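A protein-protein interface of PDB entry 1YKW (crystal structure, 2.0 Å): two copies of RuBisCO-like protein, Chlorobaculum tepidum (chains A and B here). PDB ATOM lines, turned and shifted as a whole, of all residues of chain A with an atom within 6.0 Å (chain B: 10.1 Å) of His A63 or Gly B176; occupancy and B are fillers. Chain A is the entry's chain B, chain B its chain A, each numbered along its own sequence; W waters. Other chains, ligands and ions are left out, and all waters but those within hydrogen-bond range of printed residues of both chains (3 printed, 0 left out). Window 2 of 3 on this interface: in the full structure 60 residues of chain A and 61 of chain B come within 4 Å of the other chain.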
ATOM      1  N   SER A  46      -9.828  -9.329  -5.091  1.00  0.00           N
ATOM      2  CA  SER A  46      -9.494  -8.926  -3.732  1.00  0.00           C
ATOM      3  C   SER A  46      -8.377  -7.877  -3.766  1.00  0.00           C
ATOM      4  O   SER A  46      -8.593  -6.751  -4.197  1.00  0.00           O
ATOM      5  CB  SER A  46      -9.157 -10.164  -2.876  1.00  0.00           C
ATOM      6  OG  SER A  46      -8.279 -11.071  -3.543  1.00  0.00           O
ATOM      7  N   THR A  47      -7.187  -8.257  -3.319  1.00  0.00           N
ATOM      8  CA  THR A  47      -6.008  -7.391  -3.305  1.00  0.00           C
ATOM      9  C   THR A  47      -5.313  -7.312  -4.683  1.00  0.00           C
ATOM     10  O   THR A  47      -4.434  -8.129  -5.018  1.00  0.00           O
ATOM     11  CB  THR A  47      -5.001  -7.930  -2.279  1.00  0.00           C
ATOM     12  OG1 THR A  47      -4.740  -9.306  -2.597  1.00  0.00           O
ATOM     13  CG2 THR A  47      -5.581  -7.836  -0.860  1.00  0.00           C
ATOM     14  N   ARG A  60      -2.347  -9.552   0.896  1.00  0.00           N
ATOM     15  CA  ARG A  60      -2.665  -9.440   2.321  1.00  0.00           C
ATOM     16  C   ARG A  60      -3.231 -10.777   2.830  1.00  0.00           C
ATOM     17  O   ARG A  60      -4.141 -11.366   2.226  1.00  0.00           O
ATOM     18  CB  ARG A  60      -3.659  -8.299   2.603  1.00  0.00           C
ATOM     19  CG  ARG A  60      -3.298  -6.929   1.999  1.00  0.00           C
ATOM     20  CD  ARG A  60      -2.706  -5.941   3.002  1.00  0.00           C
ATOM     21  NE  ARG A  60      -2.491  -4.621   2.400  1.00  0.00           N
ATOM     22  CZ  ARG A  60      -1.689  -3.672   2.889  1.00  0.00           C
ATOM     23  NH1 ARG A  60      -0.995  -3.870   4.004  1.00  0.00           N
ATOM     24  NH2 ARG A  60      -1.567  -2.511   2.255  1.00  0.00           N
ATOM     25  N   LEU A  61      -2.657 -11.250   3.936  1.00  0.00           N
ATOM     26  CA  LEU A  61      -3.051 -12.501   4.582  1.00  0.00           C
ATOM     27  C   LEU A  61      -4.529 -12.464   5.010  1.00  0.00           C
ATOM     28  O   LEU A  61      -5.251 -13.460   4.889  1.00  0.00           O
ATOM     29  CB  LEU A  61      -2.115 -12.792   5.770  1.00  0.00           C
ATOM     30  CG  LEU A  61      -0.608 -12.490   5.621  1.00  0.00           C
ATOM     31  CD1 LEU A  61       0.180 -12.814   6.895  1.00  0.00           C
ATOM     32  CD2 LEU A  61       0.034 -13.178   4.414  1.00  0.00           C
ATOM     33  N   VAL A  62      -4.964 -11.293   5.475  1.00  0.00           N
ATOM     34  CA  VAL A  62      -6.348 -11.014   5.891  1.00  0.00           C
ATOM     35  C   VAL A  62      -7.338 -10.723   4.739  1.00  0.00           C
ATOM     36  O   VAL A  62      -8.532 -11.017   4.858  1.00  0.00           O
ATOM     37  CB  VAL A  62      -6.362  -9.855   6.937  1.00  0.00           C
ATOM     38  CG1 VAL A  62      -5.441  -8.726   6.506  1.00  0.00           C
ATOM     39  CG2 VAL A  62      -7.768  -9.329   7.204  1.00  0.00           C
ATOM     40  N   HIS A  63      -6.845 -10.176   3.625  1.00  0.00           N
ATOM     41  CA  HIS A  63      -7.712  -9.600   2.587  1.00  0.00           C
ATOM     42  C   HIS A  63      -7.679 -10.315   1.246  1.00  0.00           C
ATOM     43  O   HIS A  63      -8.544 -10.050   0.405  1.00  0.00           O
ATOM     44  CB  HIS A  63      -7.426  -8.105   2.352  1.00  0.00           C
ATOM     45  CG  HIS A  63      -7.677  -7.239   3.547  1.00  0.00           C
ATOM     46  ND1 HIS A  63      -6.664  -6.597   4.223  1.00  0.00           N
ATOM     47  CD2 HIS A  63      -8.824  -6.923   4.198  1.00  0.00           C
ATOM     48  CE1 HIS A  63      -7.173  -5.917   5.237  1.00  0.00           C
ATOM     49  NE2 HIS A  63      -8.481  -6.103   5.248  1.00  0.00           N
ATOM     50  N   ALA A  64      -6.707 -11.203   1.028  1.00  0.00           N
ATOM     51  CA  ALA A  64      -6.713 -11.969  -0.216  1.00  0.00           C
ATOM     52  C   ALA A  64      -7.709 -13.134  -0.231  1.00  0.00           C
ATOM     53  O   ALA A  64      -7.773 -13.915   0.716  1.00  0.00           O
ATOM     54  CB  ALA A  64      -5.313 -12.463  -0.595  1.00  0.00           C
ATOM     55  N   ALA A  65      -8.473 -13.224  -1.320  1.00  0.00           N
ATOM     56  CA  ALA A  65      -9.127 -14.455  -1.724  1.00  0.00           C
ATOM     57  C   ALA A  65      -8.048 -15.489  -2.072  1.00  0.00           C
ATOM     58  O   ALA A  65      -6.984 -15.136  -2.632  1.00  0.00           O
ATOM     59  CB  ALA A  65     -10.066 -14.217  -2.916  1.00  0.00           C
ATOM     60  N   HIS A 100     -12.988 -16.778   0.172  1.00  0.00           N
ATOM     61  CA  HIS A 100     -13.027 -15.337   0.027  1.00  0.00           C
ATOM     62  C   HIS A 100     -13.365 -14.703   1.371  1.00  0.00           C
ATOM     63  O   HIS A 100     -14.444 -14.941   1.901  1.00  0.00           O
ATOM     64  CB  HIS A 100     -14.084 -14.934  -1.017  1.00  0.00           C
ATOM     65  CG  HIS A 100     -13.864 -13.575  -1.605  1.00  0.00           C
ATOM     66  ND1 HIS A 100     -13.948 -13.327  -2.958  1.00  0.00           N
ATOM     67  CD2 HIS A 100     -13.541 -12.396  -1.021  1.00  0.00           C
ATOM     68  CE1 HIS A 100     -13.690 -12.049  -3.181  1.00  0.00           C
ATOM     69  NE2 HIS A 100     -13.414 -11.467  -2.026  1.00  0.00           N
ATOM     70  N   PRO A 101     -12.431 -13.917   1.943  1.00  0.00           N
ATOM     71  CA  PRO A 101     -12.648 -13.356   3.272  1.00  0.00           C
ATOM     72  C   PRO A 101     -13.784 -12.351   3.299  1.00  0.00           C
ATOM     73  O   PRO A 101     -13.736 -11.354   2.555  1.00  0.00           O
ATOM     74  CB  PRO A 101     -11.339 -12.644   3.586  1.00  0.00           C
ATOM     75  CG  PRO A 101     -10.691 -12.429   2.265  1.00  0.00           C
ATOM     76  CD  PRO A 101     -11.108 -13.546   1.396  1.00  0.00           C
ATOM     77  N   CYS A 103     -14.743 -10.266   5.560  1.00  0.00           N
ATOM     78  CA  CYS A 103     -14.378  -8.942   6.080  1.00  0.00           C
ATOM     79  C   CYS A 103     -14.223  -7.865   4.985  1.00  0.00           C
ATOM     80  O   CYS A 103     -14.308  -6.669   5.266  1.00  0.00           O
ATOM     81  CB  CYS A 103     -13.070  -9.004   6.888  1.00  0.00           C
ATOM     82  SG  CYS A 103     -11.532  -9.097   5.884  1.00  0.00           S
ATOM     83  N   ASN A 104     -13.950  -8.283   3.758  1.00  0.00           N
ATOM     84  CA  ASN A 104     -13.811  -7.354   2.637  1.00  0.00           C
ATOM     85  C   ASN A 104     -15.123  -6.646   2.228  1.00  0.00           C
ATOM     86  O   ASN A 104     -15.108  -5.523   1.708  1.00  0.00           O
ATOM     87  CB  ASN A 104     -13.228  -8.110   1.445  1.00  0.00           C
ATOM     88  CG  ASN A 104     -11.762  -8.418   1.617  1.00  0.00           C
ATOM     89  OD1 ASN A 104     -11.129  -7.947   2.556  1.00  0.00           O
ATOM     90  ND2 ASN A 104     -11.209  -9.194   0.699  1.00  0.00           N
ATOM     91  N   VAL B 171      -6.687   5.374  -6.421  1.00  0.00           N
ATOM     92  CA  VAL B 171      -5.650   5.379  -5.395  1.00  0.00           C
ATOM     93  C   VAL B 171      -5.277   3.930  -5.101  1.00  0.00           C
ATOM     94  O   VAL B 171      -6.148   3.111  -4.811  1.00  0.00           O
ATOM     95  CB  VAL B 171      -6.150   6.061  -4.084  1.00  0.00           C
ATOM     96  CG1 VAL B 171      -4.983   6.343  -3.124  1.00  0.00           C
ATOM     97  CG2 VAL B 171      -6.959   7.340  -4.378  1.00  0.00           C
ATOM     98  N   LYS B 172      -3.997   3.607  -5.205  1.00  0.00           N
ATOM     99  CA  LYS B 172      -3.566   2.217  -5.074  1.00  0.00           C
ATOM    100  C   LYS B 172      -2.186   2.123  -4.427  1.00  0.00           C
ATOM    101  O   LYS B 172      -1.334   2.963  -4.730  1.00  0.00           O
ATOM    102  CB  LYS B 172      -3.622   1.525  -6.442  1.00  0.00           C
ATOM    103  CG  LYS B 172      -4.902   0.715  -6.614  1.00  0.00           C
ATOM    104  CD  LYS B 172      -5.543   0.831  -7.987  1.00  0.00           C
ATOM    105  CE  LYS B 172      -6.806  -0.028  -8.021  1.00  0.00           C
ATOM    106  NZ  LYS B 172      -7.570   0.111  -9.294  1.00  0.00           N
ATOM    107  N   PRO B 173      -1.946   1.103  -3.558  1.00  0.00           N
ATOM    108  CA  PRO B 173      -2.696  -0.133  -3.190  1.00  0.00           C
ATOM    109  C   PRO B 173      -4.166  -0.026  -2.742  1.00  0.00           C
ATOM    110  O   PRO B 173      -4.490   0.597  -1.721  1.00  0.00           O
ATOM    111  CB  PRO B 173      -1.837  -0.783  -2.093  1.00  0.00           C
ATOM    112  CG  PRO B 173      -0.872   0.266  -1.657  1.00  0.00           C
ATOM    113  CD  PRO B 173      -0.672   1.193  -2.822  1.00  0.00           C
ATOM    114  N   ASN B 174      -5.018  -0.699  -3.513  1.00  0.00           N
ATOM    115  CA  ASN B 174      -6.487  -0.606  -3.467  1.00  0.00           C
ATOM    116  C   ASN B 174      -7.168  -0.791  -2.098  1.00  0.00           C
ATOM    117  O   ASN B 174      -7.874   0.110  -1.627  1.00  0.00           O
ATOM    118  CB  ASN B 174      -7.091  -1.573  -4.505  1.00  0.00           C
ATOM    119  CG  ASN B 174      -6.369  -2.939  -4.550  1.00  0.00           C
ATOM    120  OD1 ASN B 174      -5.150  -3.015  -4.753  1.00  0.00           O
ATOM    121  ND2 ASN B 174      -7.134  -4.020  -4.372  1.00  0.00           N
ATOM    122  N   ILE B 175      -6.933  -1.954  -1.480  1.00  0.00           N
ATOM    123  CA  ILE B 175      -7.579  -2.394  -0.236  1.00  0.00           C
ATOM    124  C   ILE B 175      -6.538  -2.690   0.859  1.00  0.00           C
ATOM    125  O   ILE B 175      -5.412  -3.107   0.568  1.00  0.00           O
ATOM    126  CB  ILE B 175      -8.432  -3.696  -0.460  1.00  0.00           C
ATOM    127  CG1 ILE B 175      -9.156  -3.722  -1.825  1.00  0.00           C
ATOM    128  CG2 ILE B 175      -9.388  -3.962   0.712  1.00  0.00           C
ATOM    129  CD1 ILE B 175     -10.224  -2.665  -2.057  1.00  0.00           C
ATOM    130  N   GLY B 176      -6.929  -2.478   2.114  1.00  0.00           N
ATOM    131  CA  GLY B 176      -6.125  -2.875   3.268  1.00  0.00           C
ATOM    132  C   GLY B 176      -5.164  -1.824   3.792  1.00  0.00           C
ATOM    133  O   GLY B 176      -4.260  -2.136   4.575  1.00  0.00           O
ATOM    134  N   LEU B 177      -5.357  -0.582   3.354  1.00  0.00           N
ATOM    135  CA  LEU B 177      -4.533   0.542   3.796  1.00  0.00           C
ATOM    136  C   LEU B 177      -5.210   1.319   4.927  1.00  0.00           C
ATOM    137  O   LEU B 177      -6.428   1.182   5.138  1.00  0.00           O
ATOM    138  CB  LEU B 177      -4.235   1.486   2.622  1.00  0.00           C
ATOM    139  CG  LEU B 177      -3.105   1.144   1.646  1.00  0.00           C
ATOM    140  CD1 LEU B 177      -2.982   2.249   0.600  1.00  0.00           C
ATOM    141  CD2 LEU B 177      -1.778   0.939   2.368  1.00  0.00           C
ATOM    142  N   SER B 178      -4.414   2.110   5.652  1.00  0.00           N
ATOM    143  CA  SER B 178      -4.938   3.128   6.569  1.00  0.00           C
ATOM    144  C   SER B 178      -5.547   4.267   5.763  1.00  0.00           C
ATOM    145  O   SER B 178      -5.019   4.616   4.704  1.00  0.00           O
ATOM    146  CB  SER B 178      -3.837   3.722   7.456  1.00  0.00           C
ATOM    147  OG  SER B 178      -3.370   2.806   8.430  1.00  0.00           O
ATOM    148  N   PRO B 179      -6.666   4.837   6.250  1.00  0.00           N
ATOM    149  CA  PRO B 179      -7.182   6.126   5.769  1.00  0.00           C
ATOM    150  C   PRO B 179      -6.156   7.272   5.738  1.00  0.00           C
ATOM    151  O   PRO B 179      -6.289   8.176   4.912  1.00  0.00           O
ATOM    152  CB  PRO B 179      -8.315   6.433   6.754  1.00  0.00           C
ATOM    153  CG  PRO B 179      -8.815   5.067   7.152  1.00  0.00           C
ATOM    154  CD  PRO B 179      -7.563   4.236   7.259  1.00  0.00           C
ATOM    155  N   GLY B 180      -5.156   7.234   6.619  1.00  0.00           N
ATOM    156  CA  GLY B 180      -4.069   8.222   6.626  1.00  0.00           C
ATOM    157  C   GLY B 180      -2.990   7.925   5.598  1.00  0.00           C
ATOM    158  O   GLY B 180      -2.364   8.841   5.055  1.00  0.00           O
ATOM    159  N   GLU B 181      -2.765   6.637   5.349  1.00  0.00           N
ATOM    160  CA  GLU B 181      -1.872   6.175   4.287  1.00  0.00           C
ATOM    161  C   GLU B 181      -2.450   6.505   2.913  1.00  0.00           C
ATOM    162  O   GLU B 181      -1.760   7.056   2.058  1.00  0.00           O
ATOM    163  CB  GLU B 181      -1.629   4.669   4.417  1.00  0.00           C
ATOM    164  CG  GLU B 181      -0.748   4.299   5.609  1.00  0.00           C
ATOM    165  CD  GLU B 181      -1.064   2.928   6.191  1.00  0.00           C
ATOM    166  OE1 GLU B 181      -0.715   2.696   7.372  1.00  0.00           O
ATOM    167  OE2 GLU B 181      -1.663   2.088   5.483  1.00  0.00           O
ATOM    168  N   PHE B 182      -3.724   6.156   2.728  1.00  0.00           N
ATOM    169  CA  PHE B 182      -4.518   6.483   1.546  1.00  0.00           C
ATOM    170  C   PHE B 182      -4.368   7.969   1.234  1.00  0.00           C
ATOM    171  O   PHE B 182      -3.976   8.342   0.136  1.00  0.00           O
ATOM    172  CB  PHE B 182      -5.984   6.172   1.863  1.00  0.00           C
ATOM    173  CG  PHE B 182      -6.801   5.713   0.686  1.00  0.00           C
ATOM    174  CD1 PHE B 182      -6.954   4.351   0.421  1.00  0.00           C
ATOM    175  CD2 PHE B 182      -7.476   6.634  -0.117  1.00  0.00           C
ATOM    176  CE1 PHE B 182      -7.740   3.911  -0.651  1.00  0.00           C
ATOM    177  CE2 PHE B 182      -8.273   6.211  -1.198  1.00  0.00           C
ATOM    178  CZ  PHE B 182      -8.408   4.844  -1.463  1.00  0.00           C
ATOM    179  N   ILE B 185      -1.057   9.541  -0.542  1.00  0.00           N
ATOM    180  CA  ILE B 185      -0.947   9.173  -1.956  1.00  0.00           C
ATOM    181  C   ILE B 185      -1.920   9.986  -2.822  1.00  0.00           C
ATOM    182  O   ILE B 185      -1.530  10.504  -3.886  1.00  0.00           O
ATOM    183  CB  ILE B 185      -1.123   7.649  -2.152  1.00  0.00           C
ATOM    184  CG1 ILE B 185      -0.069   6.896  -1.329  1.00  0.00           C
ATOM    185  CG2 ILE B 185      -0.982   7.265  -3.623  1.00  0.00           C
ATOM    186  CD1 ILE B 185      -0.562   5.621  -0.654  1.00  0.00           C
ATOM    187  N   ASP B 200     -11.484   2.572  -4.423  1.00  0.00           N
ATOM    188  CA  ASP B 200     -11.708   1.315  -5.143  1.00  0.00           C
ATOM    189  C   ASP B 200     -13.182   0.885  -5.049  1.00  0.00           C
ATOM    190  O   ASP B 200     -13.816   1.037  -4.000  1.00  0.00           O
ATOM    191  CB  ASP B 200     -10.810   0.210  -4.574  1.00  0.00           C
ATOM    192  CG  ASP B 200     -10.546  -0.896  -5.583  1.00  0.00           C
ATOM    193  OD1 ASP B 200      -9.653  -0.704  -6.443  1.00  0.00           O
ATOM    194  OD2 ASP B 200     -11.230  -1.944  -5.527  1.00  0.00           O
ATOM    195  N   MET B 202     -14.375  -1.899  -4.690  1.00  0.00           N
ATOM    196  CA  MET B 202     -14.462  -2.953  -3.677  1.00  0.00           C
ATOM    197  C   MET B 202     -14.105  -2.481  -2.252  1.00  0.00           C
ATOM    198  O   MET B 202     -14.012  -3.292  -1.315  1.00  0.00           O
ATOM    199  CB  MET B 202     -13.568  -4.136  -4.073  1.00  0.00           C
ATOM    200  CG  MET B 202     -13.968  -4.845  -5.371  1.00  0.00           C
ATOM    201  SD  MET B 202     -13.259  -6.508  -5.435  1.00  0.00           S
ATOM    202  CE  MET B 202     -11.497  -6.123  -5.503  1.00  0.00           C
ATOM    203  N   LEU B 203     -13.881  -1.180  -2.080  1.00  0.00           N
ATOM    204  CA  LEU B 203     -13.625  -0.647  -0.743  1.00  0.00           C
ATOM    205  C   LEU B 203     -14.673   0.388  -0.355  1.00  0.00           C
ATOM    206  O   LEU B 203     -14.504   1.569  -0.657  1.00  0.00           O
ATOM    207  CB  LEU B 203     -12.215  -0.041  -0.618  1.00  0.00           C
ATOM    208  CG  LEU B 203     -11.752   0.444   0.771  1.00  0.00           C
ATOM    209  CD1 LEU B 203     -11.126  -0.692   1.609  1.00  0.00           C
ATOM    210  CD2 LEU B 203     -10.782   1.638   0.660  1.00  0.00           C
ATOM    211  N   ALA B 204     -15.742  -0.053   0.312  1.00  0.00           N
ATOM    212  CA  ALA B 204     -16.751   0.871   0.824  1.00  0.00           C
ATOM    213  C   ALA B 204     -16.634   1.053   2.343  1.00  0.00           C
ATOM    214  O   ALA B 204     -15.559   1.389   2.852  1.00  0.00           O
ATOM    215  CB  ALA B 204     -18.154   0.431   0.407  1.00  0.00           C
ATOM    216  N   VAL B 206     -16.213  -0.482   5.690  1.00  0.00           N
ATOM    217  CA  VAL B 206     -15.769  -1.704   6.362  1.00  0.00           C
ATOM    218  C   VAL B 206     -15.008  -1.357   7.646  1.00  0.00           C
ATOM    219  O   VAL B 206     -14.630  -0.211   7.865  1.00  0.00           O
ATOM    220  CB  VAL B 206     -14.897  -2.609   5.443  1.00  0.00           C
ATOM    221  CG1 VAL B 206     -15.631  -2.946   4.147  1.00  0.00           C
ATOM    222  CG2 VAL B 206     -13.546  -1.959   5.144  1.00  0.00           C
ATOM    223  N   THR B 207     -14.758  -2.368   8.469  1.00  0.00           N
ATOM    224  CA  THR B 207     -14.297  -2.176   9.850  1.00  0.00           C
ATOM    225  C   THR B 207     -12.905  -1.567  10.085  1.00  0.00           C
ATOM    226  O   THR B 207     -12.739  -0.800  11.036  1.00  0.00           O
ATOM    227  CB  THR B 207     -14.463  -3.478  10.673  1.00  0.00           C
ATOM    228  OG1 THR B 207     -13.765  -4.547  10.023  1.00  0.00           O
ATOM    229  CG2 THR B 207     -15.948  -3.844  10.792  1.00  0.00           C
ATOM    230  N   TRP B 208     -11.910  -1.915   9.263  1.00  0.00           N
ATOM    231  CA  TRP B 208     -10.563  -1.317   9.368  1.00  0.00           C
ATOM    232  C   TRP B 208     -10.439  -0.001   8.573  1.00  0.00           C
ATOM    233  O   TRP B 208      -9.401   0.675   8.623  1.00  0.00           O
ATOM    234  CB  TRP B 208      -9.480  -2.301   8.896  1.00  0.00           C
ATOM    235  CG  TRP B 208      -9.431  -2.393   7.390  1.00  0.00           C
ATOM    236  CD1 TRP B 208      -8.647  -1.655   6.541  1.00  0.00           C
ATOM    237  CD2 TRP B 208     -10.235  -3.240   6.558  1.00  0.00           C
ATOM    238  NE1 TRP B 208      -8.907  -1.999   5.233  1.00  0.00           N
ATOM    239  CE2 TRP B 208      -9.874  -2.970   5.213  1.00  0.00           C
ATOM    240  CE3 TRP B 208     -11.220  -4.208   6.817  1.00  0.00           C
ATOM    241  CZ2 TRP B 208     -10.456  -3.639   4.134  1.00  0.00           C
ATOM    242  CZ3 TRP B 208     -11.804  -4.867   5.745  1.00  0.00           C
ATOM    243  CH2 TRP B 208     -11.415  -4.583   4.420  1.00  0.00           C
ATOM    244  N   SER B 209     -11.488   0.331   7.819  1.00  0.00           N
ATOM    245  CA  SER B 209     -11.540   1.537   6.987  1.00  0.00           C
ATOM    246  C   SER B 209     -12.995   1.997   6.842  1.00  0.00           C
ATOM    247  O   SER B 209     -13.650   1.733   5.831  1.00  0.00           O
ATOM    248  CB  SER B 209     -10.892   1.275   5.621  1.00  0.00           C
ATOM    249  OG  SER B 209     -10.762   2.475   4.879  1.00  0.00           O
ATOM    250  N   ARG B 214     -12.109   7.421   6.614  1.00  0.00           N
ATOM    251  CA  ARG B 214     -11.588   7.745   5.286  1.00  0.00           C
ATOM    252  C   ARG B 214     -11.969   9.169   4.899  1.00  0.00           C
ATOM    253  O   ARG B 214     -11.097   9.975   4.610  1.00  0.00           O
ATOM    254  CB  ARG B 214     -12.054   6.766   4.197  1.00  0.00           C
ATOM    255  CG  ARG B 214     -11.078   5.629   3.950  1.00  0.00           C
ATOM    256  CD  ARG B 214     -11.183   5.009   2.553  1.00  0.00           C
ATOM    257  NE  ARG B 214     -12.561   4.885   2.057  1.00  0.00           N
ATOM    258  CZ  ARG B 214     -13.460   3.994   2.476  1.00  0.00           C
ATOM    259  NH1 ARG B 214     -13.150   3.117   3.422  1.00  0.00           N
ATOM    260  NH2 ARG B 214     -14.684   3.984   1.945  1.00  0.00           N
HETATM  261  O   HOH W   1     -14.855  -6.478  -1.588  1.00  0.00           O
HETATM  262  O   HOH W   2     -16.519  -3.014   1.039  1.00  0.00           O
HETATM  263  O   HOH W   3     -12.801  -3.909   0.970  1.00  0.00           O
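Water W3 bridges O of Met B202 and O of Asn A104. Water W2 lies within hydrogen-bond range of O of Asn A104 (3.0 Å), N of Ala B204 (3.1 Å) and O of Met B202 (3.5 Å). Water W1 lies within hydrogen-bond range of the backbone carbonyl oxygen of Met B202 (3.3 Å) and the backbone carbonyl oxygen of Asn A104 (3.4 Å).
Of the printed residues of chain B, Thr A47 touches Asn B174 (3.7 Å). Of the printed residues of chain B, Arg A60 touches Ile B175 (3.8 Å), Gly B176 (3.4 Å) and Leu B177 (3.5 Å). His A63 touches two residues of chain B. Of the printed residues of chain A, Asn B174 touches Ser A46 (3.1 Å) and Thr A47 (3.7 Å). Of chain A, only Arg A60 (3.4 Å) and His A63 (3.8 Å) come within 4 Å of Gly B176. Printed residues of chain A within 4 Å of Leu B177: Arg A60. Of the printed residues of chain A, Met B202 touches Ser A46 and Asn A104.
Hydrophobic or aromatic side chains of chain A that line the printed part of chain B: His A63. Of the 22 printed residues of chain B, 7 touch a printed residue of chain A. Printed residues of chain B that touch a printed residue of chain A: Asn B174, Ile B175, Gly B176, Leu B177, Met B202, Val B206 and Trp B208. Hydrophobic or aromatic side chains of chain B within 4 Å of the printed part of chain A: Ile B175, Leu B177, Met B202, Val B206 and Trp B208. Among the printed residues, no Asp or Glu carboxylate lies within 4 Å of a Lys or Arg side-chain nitrogen of the other chain.
Ser A46 touches Met B202 (O to CE, 3.2 Å). CA of Thr A47 touches ND2 of Asn B174, at 3.7 Å. Ile B175 touches Arg A60 (O to NE, 3.8 Å). CZ of Arg A60 touches O of Gly B176, 3.4 Å away. CD2 of Leu B177 touches NH2 of Arg A60, 3.5 Å away. His A63 touches Gly B176 (CE1 to CA, 3.8 Å). Trp B208 touches His A63 (CZ2 to NE2, 3.3 Å). Asn A104 touches Met B202. Asn A104 touches Val B206 (O to CG1, 3.6 Å). Trp B208 touches Asn A104 (CH2 to OD1, 3.9 Å).
ND2 of Asn B174 is in hydrogen-bond range of O of Ser A46.
OD2 of Asp B200 lies close to N of Met B202, 3.3 Å away. The side-chain hydroxyl (OG) of Ser A46 lies within hydrogen-bond range of the backbone NH (N) of Ala A65 (3.1 Å). The backbone carbonyl oxygen of Val A62 sits at hydrogen-bond distance from the side-chain sulfur of Cys A103. O of His A63 is in hydrogen-bond range of ND2 of Asn A104. The side-chain sulfur (SG) of Cys A103 is in hydrogen-bond range of the side-chain amide oxygen (OD1) of Asn A104 (3.5 Å).
No position is printed for both chains.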
